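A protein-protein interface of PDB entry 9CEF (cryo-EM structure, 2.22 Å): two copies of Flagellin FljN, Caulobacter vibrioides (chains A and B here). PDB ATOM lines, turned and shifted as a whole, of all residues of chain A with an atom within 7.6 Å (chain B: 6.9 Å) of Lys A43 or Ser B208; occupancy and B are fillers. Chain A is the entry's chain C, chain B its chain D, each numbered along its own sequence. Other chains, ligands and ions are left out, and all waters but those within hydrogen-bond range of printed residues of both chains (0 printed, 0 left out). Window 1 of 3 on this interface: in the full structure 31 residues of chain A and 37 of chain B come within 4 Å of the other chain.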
ATOM      1  N   GLN A  31      10.508 -14.758 -34.559  1.00  0.00           N
ATOM      2  CA  GLN A  31      11.146 -13.610 -33.921  1.00  0.00           C
ATOM      3  C   GLN A  31      12.255 -14.040 -32.971  1.00  0.00           C
ATOM      4  O   GLN A  31      13.309 -13.397 -32.908  1.00  0.00           O
ATOM      5  CB  GLN A  31      10.121 -12.768 -33.180  1.00  0.00           C
ATOM      6  CG  GLN A  31       9.127 -12.098 -34.072  1.00  0.00           C
ATOM      7  CD  GLN A  31       8.009 -11.465 -33.286  1.00  0.00           C
ATOM      8  OE1 GLN A  31       7.352 -12.119 -32.485  1.00  0.00           O
ATOM      9  NE2 GLN A  31       7.799 -10.178 -33.497  1.00  0.00           N
ATOM     10  N   ILE A  39      12.906 -12.430 -24.914  1.00  0.00           N
ATOM     11  CA  ILE A  39      12.289 -11.160 -24.540  1.00  0.00           C
ATOM     12  C   ILE A  39      13.016 -10.081 -25.332  1.00  0.00           C
ATOM     13  O   ILE A  39      14.042  -9.548 -24.914  1.00  0.00           O
ATOM     14  CB  ILE A  39      12.339 -10.900 -23.033  1.00  0.00           C
ATOM     15  CG1 ILE A  39      11.469 -11.921 -22.301  1.00  0.00           C
ATOM     16  CG2 ILE A  39      11.886  -9.487 -22.709  1.00  0.00           C
ATOM     17  CD1 ILE A  39      11.923 -12.258 -20.931  1.00  0.00           C
ATOM     18  N   GLY A  40      12.499  -9.773 -26.512  1.00  0.00           N
ATOM     19  CA  GLY A  40      13.158  -8.835 -27.391  1.00  0.00           C
ATOM     20  C   GLY A  40      12.576  -7.444 -27.392  1.00  0.00           C
ATOM     21  O   GLY A  40      13.166  -6.529 -27.962  1.00  0.00           O
ATOM     22  N   SER A  41      11.433  -7.261 -26.749  1.00  0.00           N
ATOM     23  CA  SER A  41      10.772  -5.965 -26.731  1.00  0.00           C
ATOM     24  C   SER A  41       9.884  -5.897 -25.502  1.00  0.00           C
ATOM     25  O   SER A  41       9.666  -6.892 -24.814  1.00  0.00           O
ATOM     26  CB  SER A  41       9.970  -5.727 -28.013  1.00  0.00           C
ATOM     27  OG  SER A  41       8.739  -6.411 -27.999  1.00  0.00           O
ATOM     28  N   ALA A  42       9.378  -4.698 -25.234  1.00  0.00           N
ATOM     29  CA  ALA A  42       8.467  -4.493 -24.120  1.00  0.00           C
ATOM     30  C   ALA A  42       7.171  -5.276 -24.279  1.00  0.00           C
ATOM     31  O   ALA A  42       6.492  -5.531 -23.285  1.00  0.00           O
ATOM     32  CB  ALA A  42       8.179  -3.003 -23.961  1.00  0.00           C
ATOM     33  N   LYS A  43       6.806  -5.644 -25.504  1.00  0.00           N
ATOM     34  CA  LYS A  43       5.613  -6.454 -25.721  1.00  0.00           C
ATOM     35  C   LYS A  43       5.760  -7.883 -25.199  1.00  0.00           C
ATOM     36  O   LYS A  43       4.756  -8.509 -24.860  1.00  0.00           O
ATOM     37  CB  LYS A  43       5.258  -6.465 -27.205  1.00  0.00           C
ATOM     38  CG  LYS A  43       4.464  -5.265 -27.640  1.00  0.00           C
ATOM     39  CD  LYS A  43       4.241  -5.219 -29.133  1.00  0.00           C
ATOM     40  CE  LYS A  43       5.532  -5.087 -29.892  1.00  0.00           C
ATOM     41  NZ  LYS A  43       5.662  -6.128 -30.931  1.00  0.00           N
ATOM     42  N   ASP A  44       6.977  -8.427 -25.131  1.00  0.00           N
ATOM     43  CA  ASP A  44       7.126  -9.815 -24.689  1.00  0.00           C
ATOM     44  C   ASP A  44       6.913  -9.971 -23.187  1.00  0.00           C
ATOM     45  O   ASP A  44       6.282 -10.936 -22.748  1.00  0.00           O
ATOM     46  CB  ASP A  44       8.491 -10.371 -25.091  1.00  0.00           C
ATOM     47  CG  ASP A  44       8.704 -10.374 -26.584  1.00  0.00           C
ATOM     48  OD1 ASP A  44       7.772 -10.756 -27.312  1.00  0.00           O
ATOM     49  OD2 ASP A  44       9.802 -10.014 -27.039  1.00  0.00           O
ATOM     50  N   ASN A  45       7.426  -9.041 -22.387  1.00  0.00           N
ATOM     51  CA  ASN A  45       7.400  -9.114 -20.928  1.00  0.00           C
ATOM     52  C   ASN A  45       7.936  -7.805 -20.379  1.00  0.00           C
ATOM     53  O   ASN A  45       9.149  -7.648 -20.248  1.00  0.00           O
ATOM     54  CB  ASN A  45       8.238 -10.291 -20.419  1.00  0.00           C
ATOM     55  CG  ASN A  45       8.068 -10.548 -18.932  1.00  0.00           C
ATOM     56  OD1 ASN A  45       8.008  -9.628 -18.131  1.00  0.00           O
ATOM     57  ND2 ASN A  45       8.022 -11.804 -18.562  1.00  0.00           N
ATOM     58  N   GLY A  46       7.052  -6.867 -20.049  1.00  0.00           N
ATOM     59  CA  GLY A  46       7.493  -5.500 -19.840  1.00  0.00           C
ATOM     60  C   GLY A  46       8.421  -5.333 -18.655  1.00  0.00           C
ATOM     61  O   GLY A  46       9.408  -4.604 -18.734  1.00  0.00           O
ATOM     62  N   TRP A  49      11.848  -6.916 -19.410  1.00  0.00           N
ATOM     63  CA  TRP A  49      12.479  -6.104 -20.441  1.00  0.00           C
ATOM     64  C   TRP A  49      13.036  -4.811 -19.858  1.00  0.00           C
ATOM     65  O   TRP A  49      14.161  -4.415 -20.180  1.00  0.00           O
ATOM     66  CB  TRP A  49      11.476  -5.811 -21.555  1.00  0.00           C
ATOM     67  CG  TRP A  49      11.973  -4.876 -22.599  1.00  0.00           C
ATOM     68  CD1 TRP A  49      12.666  -5.197 -23.715  1.00  0.00           C
ATOM     69  CD2 TRP A  49      11.831  -3.457 -22.610  1.00  0.00           C
ATOM     70  NE1 TRP A  49      12.953  -4.079 -24.432  1.00  0.00           N
ATOM     71  CE2 TRP A  49      12.452  -2.991 -23.774  1.00  0.00           C
ATOM     72  CE3 TRP A  49      11.234  -2.537 -21.751  1.00  0.00           C
ATOM     73  CZ2 TRP A  49      12.496  -1.644 -24.104  1.00  0.00           C
ATOM     74  CZ3 TRP A  49      11.281  -1.206 -22.075  1.00  0.00           C
ATOM     75  CH2 TRP A  49      11.910  -0.768 -23.240  1.00  0.00           C
ATOM     76  N   GLY B  72      -4.707   0.798 -33.001  1.00  0.00           N
ATOM     77  CA  GLY B  72      -4.045   1.039 -31.734  1.00  0.00           C
ATOM     78  C   GLY B  72      -2.725   0.309 -31.619  1.00  0.00           C
ATOM     79  O   GLY B  72      -1.746   0.851 -31.094  1.00  0.00           O
ATOM     80  N   GLN B  73      -2.666  -0.914 -32.143  1.00  0.00           N
ATOM     81  CA  GLN B  73      -1.402  -1.638 -32.126  1.00  0.00           C
ATOM     82  C   GLN B  73      -0.352  -0.943 -32.991  1.00  0.00           C
ATOM     83  O   GLN B  73       0.823  -0.883 -32.618  1.00  0.00           O
ATOM     84  CB  GLN B  73      -1.621  -3.081 -32.578  1.00  0.00           C
ATOM     85  CG  GLN B  73      -2.072  -4.010 -31.463  1.00  0.00           C
ATOM     86  CD  GLN B  73      -2.504  -5.375 -31.957  1.00  0.00           C
ATOM     87  OE1 GLN B  73      -3.661  -5.589 -32.275  1.00  0.00           O
ATOM     88  NE2 GLN B  73      -1.580  -6.312 -31.981  1.00  0.00           N
ATOM     89  N   SER B  74      -0.766  -0.357 -34.120  1.00  0.00           N
ATOM     90  CA  SER B  74       0.185   0.378 -34.958  1.00  0.00           C
ATOM     91  C   SER B  74       0.708   1.635 -34.265  1.00  0.00           C
ATOM     92  O   SER B  74       1.907   1.946 -34.344  1.00  0.00           O
ATOM     93  CB  SER B  74      -0.459   0.752 -36.287  1.00  0.00           C
ATOM     94  OG  SER B  74      -0.741  -0.377 -37.074  1.00  0.00           O
ATOM     95  N   ILE B  76       1.012   2.136 -31.022  1.00  0.00           N
ATOM     96  CA  ILE B  76       1.975   1.732 -30.008  1.00  0.00           C
ATOM     97  C   ILE B  76       3.279   1.243 -30.634  1.00  0.00           C
ATOM     98  O   ILE B  76       4.353   1.453 -30.067  1.00  0.00           O
ATOM     99  CB  ILE B  76       1.341   0.685 -29.077  1.00  0.00           C
ATOM    100  CG1 ILE B  76       0.202   1.324 -28.284  1.00  0.00           C
ATOM    101  CG2 ILE B  76       2.373   0.098 -28.136  1.00  0.00           C
ATOM    102  CD1 ILE B  76      -0.542   0.383 -27.406  1.00  0.00           C
ATOM    103  N   ASP B  77       3.228   0.611 -31.813  1.00  0.00           N
ATOM    104  CA  ASP B  77       4.467   0.191 -32.465  1.00  0.00           C
ATOM    105  C   ASP B  77       5.348   1.385 -32.802  1.00  0.00           C
ATOM    106  O   ASP B  77       6.569   1.344 -32.603  1.00  0.00           O
ATOM    107  CB  ASP B  77       4.171  -0.595 -33.743  1.00  0.00           C
ATOM    108  CG  ASP B  77       3.959  -2.074 -33.498  1.00  0.00           C
ATOM    109  OD1 ASP B  77       4.628  -2.646 -32.618  1.00  0.00           O
ATOM    110  OD2 ASP B  77       3.133  -2.681 -34.207  1.00  0.00           O
ATOM    111  N   LEU B  80       6.988   2.601 -29.588  1.00  0.00           N
ATOM    112  CA  LEU B  80       8.092   1.759 -29.135  1.00  0.00           C
ATOM    113  C   LEU B  80       9.335   1.939 -29.997  1.00  0.00           C
ATOM    114  O   LEU B  80      10.464   1.886 -29.484  1.00  0.00           O
ATOM    115  CB  LEU B  80       7.669   0.294 -29.121  1.00  0.00           C
ATOM    116  CG  LEU B  80       6.560  -0.119 -28.156  1.00  0.00           C
ATOM    117  CD1 LEU B  80       6.157  -1.548 -28.414  1.00  0.00           C
ATOM    118  CD2 LEU B  80       6.966   0.076 -26.710  1.00  0.00           C
ATOM    119  N   PHE B 157     -11.689   0.836 -25.273  1.00  0.00           N
ATOM    120  CA  PHE B 157     -10.506   0.176 -24.736  1.00  0.00           C
ATOM    121  C   PHE B 157      -9.480   1.294 -24.585  1.00  0.00           C
ATOM    122  O   PHE B 157      -8.813   1.662 -25.554  1.00  0.00           O
ATOM    123  CB  PHE B 157     -10.033  -0.942 -25.667  1.00  0.00           C
ATOM    124  CG  PHE B 157      -8.928  -1.791 -25.107  1.00  0.00           C
ATOM    125  CD1 PHE B 157      -7.691  -1.256 -24.811  1.00  0.00           C
ATOM    126  CD2 PHE B 157      -9.130  -3.135 -24.889  1.00  0.00           C
ATOM    127  CE1 PHE B 157      -6.691  -2.040 -24.304  1.00  0.00           C
ATOM    128  CE2 PHE B 157      -8.131  -3.921 -24.382  1.00  0.00           C
ATOM    129  CZ  PHE B 157      -6.913  -3.377 -24.091  1.00  0.00           C
ATOM    130  N   VAL B 159      -6.182   3.417 -23.644  1.00  0.00           N
ATOM    131  CA  VAL B 159      -4.739   3.304 -23.473  1.00  0.00           C
ATOM    132  C   VAL B 159      -4.248   4.634 -22.926  1.00  0.00           C
ATOM    133  O   VAL B 159      -4.376   5.665 -23.589  1.00  0.00           O
ATOM    134  CB  VAL B 159      -4.018   2.948 -24.786  1.00  0.00           C
ATOM    135  CG1 VAL B 159      -2.524   2.831 -24.559  1.00  0.00           C
ATOM    136  CG2 VAL B 159      -4.562   1.663 -25.369  1.00  0.00           C
ATOM    137  N   LEU B 201       7.570   2.630 -21.352  1.00  0.00           N
ATOM    138  CA  LEU B 201       7.548   1.715 -22.483  1.00  0.00           C
ATOM    139  C   LEU B 201       7.055   0.332 -22.084  1.00  0.00           C
ATOM    140  O   LEU B 201       6.378  -0.330 -22.876  1.00  0.00           O
ATOM    141  CB  LEU B 201       8.929   1.651 -23.127  1.00  0.00           C
ATOM    142  CG  LEU B 201       9.408   2.994 -23.682  1.00  0.00           C
ATOM    143  CD1 LEU B 201      10.902   2.994 -23.921  1.00  0.00           C
ATOM    144  CD2 LEU B 201       8.665   3.341 -24.943  1.00  0.00           C
ATOM    145  N   ALA B 202       7.340  -0.106 -20.856  1.00  0.00           N
ATOM    146  CA  ALA B 202       6.798  -1.376 -20.392  1.00  0.00           C
ATOM    147  C   ALA B 202       5.277  -1.333 -20.301  1.00  0.00           C
ATOM    148  O   ALA B 202       4.598  -2.297 -20.682  1.00  0.00           O
ATOM    149  CB  ALA B 202       7.412  -1.745 -19.044  1.00  0.00           C
ATOM    150  N   SER B 203       4.715  -0.210 -19.846  1.00  0.00           N
ATOM    151  CA  SER B 203       3.257  -0.110 -19.833  1.00  0.00           C
ATOM    152  C   SER B 203       2.680  -0.092 -21.242  1.00  0.00           C
ATOM    153  O   SER B 203       1.632  -0.695 -21.491  1.00  0.00           O
ATOM    154  CB  SER B 203       2.791   1.122 -19.062  1.00  0.00           C
ATOM    155  OG  SER B 203       3.482   1.253 -17.848  1.00  0.00           O
ATOM    156  N   LEU B 204       3.341   0.584 -22.181  1.00  0.00           N
ATOM    157  CA  LEU B 204       2.823   0.576 -23.547  1.00  0.00           C
ATOM    158  C   LEU B 204       2.873  -0.822 -24.155  1.00  0.00           C
ATOM    159  O   LEU B 204       1.962  -1.218 -24.889  1.00  0.00           O
ATOM    160  CB  LEU B 204       3.588   1.570 -24.416  1.00  0.00           C
ATOM    161  CG  LEU B 204       3.320   3.055 -24.181  1.00  0.00           C
ATOM    162  CD1 LEU B 204       4.188   3.901 -25.076  1.00  0.00           C
ATOM    163  CD2 LEU B 204       1.857   3.400 -24.373  1.00  0.00           C
ATOM    164  N   GLY B 205       3.904  -1.602 -23.830  1.00  0.00           N
ATOM    165  CA  GLY B 205       3.973  -2.954 -24.357  1.00  0.00           C
ATOM    166  C   GLY B 205       2.911  -3.866 -23.774  1.00  0.00           C
ATOM    167  O   GLY B 205       2.318  -4.684 -24.489  1.00  0.00           O
ATOM    168  N   THR B 206       2.622  -3.710 -22.480  1.00  0.00           N
ATOM    169  CA  THR B 206       1.519  -4.462 -21.894  1.00  0.00           C
ATOM    170  C   THR B 206       0.177  -4.052 -22.495  1.00  0.00           C
ATOM    171  O   THR B 206      -0.695  -4.900 -22.710  1.00  0.00           O
ATOM    172  CB  THR B 206       1.511  -4.282 -20.378  1.00  0.00           C
ATOM    173  OG1 THR B 206       2.832  -4.470 -19.871  1.00  0.00           O
ATOM    174  CG2 THR B 206       0.593  -5.269 -19.725  1.00  0.00           C
ATOM    175  N   SER B 207       0.006  -2.770 -22.812  1.00  0.00           N
ATOM    176  CA  SER B 207      -1.232  -2.346 -23.458  1.00  0.00           C
ATOM    177  C   SER B 207      -1.367  -2.938 -24.852  1.00  0.00           C
ATOM    178  O   SER B 207      -2.468  -3.300 -25.275  1.00  0.00           O
ATOM    179  CB  SER B 207      -1.297  -0.826 -23.529  1.00  0.00           C
ATOM    180  OG  SER B 207      -1.589  -0.281 -22.271  1.00  0.00           O
ATOM    181  N   SER B 208      -0.262  -3.041 -25.582  1.00  0.00           N
ATOM    182  CA  SER B 208      -0.331  -3.605 -26.921  1.00  0.00           C
ATOM    183  C   SER B 208      -0.685  -5.090 -26.873  1.00  0.00           C
ATOM    184  O   SER B 208      -1.493  -5.573 -27.678  1.00  0.00           O
ATOM    185  CB  SER B 208       0.995  -3.368 -27.640  1.00  0.00           C
ATOM    186  OG  SER B 208       0.978  -3.880 -28.949  1.00  0.00           O
ATOM    187  N   THR B 209      -0.116  -5.820 -25.912  1.00  0.00           N
ATOM    188  CA  THR B 209      -0.486  -7.222 -25.757  1.00  0.00           C
ATOM    189  C   THR B 209      -1.948  -7.374 -25.346  1.00  0.00           C
ATOM    190  O   THR B 209      -2.635  -8.295 -25.806  1.00  0.00           O
ATOM    191  CB  THR B 209       0.447  -7.896 -24.753  1.00  0.00           C
ATOM    192  OG1 THR B 209       1.778  -7.865 -25.266  1.00  0.00           O
ATOM    193  CG2 THR B 209       0.065  -9.328 -24.522  1.00  0.00           C
ATOM    194  N   GLY B 210      -2.460  -6.448 -24.533  1.00  0.00           N
ATOM    195  CA  GLY B 210      -3.867  -6.499 -24.180  1.00  0.00           C
ATOM    196  C   GLY B 210      -4.784  -6.230 -25.358  1.00  0.00           C
ATOM    197  O   GLY B 210      -5.824  -6.876 -25.504  1.00  0.00           O
ATOM    198  N   LEU B 211      -4.395  -5.304 -26.234  1.00  0.00           N
ATOM    199  CA  LEU B 211      -5.179  -5.074 -27.443  1.00  0.00           C
ATOM    200  C   LEU B 211      -5.183  -6.300 -28.344  1.00  0.00           C
ATOM    201  O   LEU B 211      -6.214  -6.639 -28.927  1.00  0.00           O
ATOM    202  CB  LEU B 211      -4.643  -3.876 -28.223  1.00  0.00           C
ATOM    203  CG  LEU B 211      -4.869  -2.443 -27.769  1.00  0.00           C
ATOM    204  CD1 LEU B 211      -3.930  -1.530 -28.522  1.00  0.00           C
ATOM    205  CD2 LEU B 211      -6.286  -2.018 -27.971  1.00  0.00           C
ATOM    206  N   ASP B 212      -4.044  -6.982 -28.461  1.00  0.00           N
ATOM    207  CA  ASP B 212      -3.989  -8.174 -29.302  1.00  0.00           C
ATOM    208  C   ASP B 212      -4.866  -9.299 -28.754  1.00  0.00           C
ATOM    209  O   ASP B 212      -5.582  -9.971 -29.512  1.00  0.00           O
ATOM    210  CB  ASP B 212      -2.541  -8.636 -29.441  1.00  0.00           C
ATOM    211  CG  ASP B 212      -2.342  -9.614 -30.578  1.00  0.00           C
ATOM    212  OD1 ASP B 212      -2.924  -9.422 -31.665  1.00  0.00           O
ATOM    213  OD2 ASP B 212      -1.595 -10.589 -30.387  1.00  0.00           O
ATOM    214  N   THR B 213      -4.841  -9.502 -27.435  1.00  0.00           N
ATOM    215  CA  THR B 213      -5.701 -10.515 -26.834  1.00  0.00           C
ATOM    216  C   THR B 213      -7.177 -10.178 -27.022  1.00  0.00           C
ATOM    217  O   THR B 213      -7.992 -11.055 -27.347  1.00  0.00           O
ATOM    218  CB  THR B 213      -5.363 -10.662 -25.351  1.00  0.00           C
ATOM    219  OG1 THR B 213      -4.021 -11.132 -25.217  1.00  0.00           O
ATOM    220  CG2 THR B 213      -6.278 -11.630 -24.691  1.00  0.00           C
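Lys A43 touches just these residues of chain B: Asp B77 (3.8 Å), Leu B80 (3.9 Å), Gly B205 (3.9 Å), Ser B208 (3.5 Å) and Thr B209 (3.1 Å). Ser B208 touches just one residue of chain A: Lys A43. Printed residues of chain A within 4 Å of Asp B77: Lys A43. Of the printed residues of chain A, Thr B209 touches Lys A43 (3.1 Å). Of the printed residues of chain A, Leu B80 touches Lys A43 (3.9 Å).
No position is printed for both chains. Of the 9 pairs that touch across the chains among the printed residues, none has its exchanged pair printed and touching as well.
The backbone carbonyl oxygen (O) of Lys A43 sits at hydrogen-bond distance from the side-chain hydroxyl (OG1) of Thr B209 (3.1 Å).
The side-chain hydroxyl (OG1) of Thr B206 sits at hydrogen-bond distance from the backbone carbonyl oxygen (O) of Ala B202 (2.9 Å). O of Gly B205 is in hydrogen-bond range of OG1 of Thr B209 (3.3 Å). The backbone NH (N) of Lys A43 sits close to the side-chain hydroxyl (OG) of Ser A41, at 3.2 Å. The backbone carbonyl oxygen (O) of Thr B209 sits at hydrogen-bond distance from the side-chain hydroxyl (OG1) of Thr B213, 3.2 Å away.
Printed residues of chain A that touch a printed residue of chain B: Ala A42, Lys A43, Gly A46 and Trp A49. Hydrophobic or aromatic side chains of chain A within 4 Å of the printed part of chain B: Ala A42 and Trp A49.
Among the printed residues, merely in contact across the chains: Ala A42 with Leu B201 (3.4 Å), Ala A42 with Gly B205 (3.8 Å), Lys A43 with Asp B77 (3.8 Å), Lys A43 with Leu B80 (3.9 Å), Lys A43 with Gly B205 (3.9 Å), Lys A43 with Ser B208 (3.5 Å), Gly A46 with Ala B202 (3.5 Å) and Trp A49 with Leu B201 (3.8 Å).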
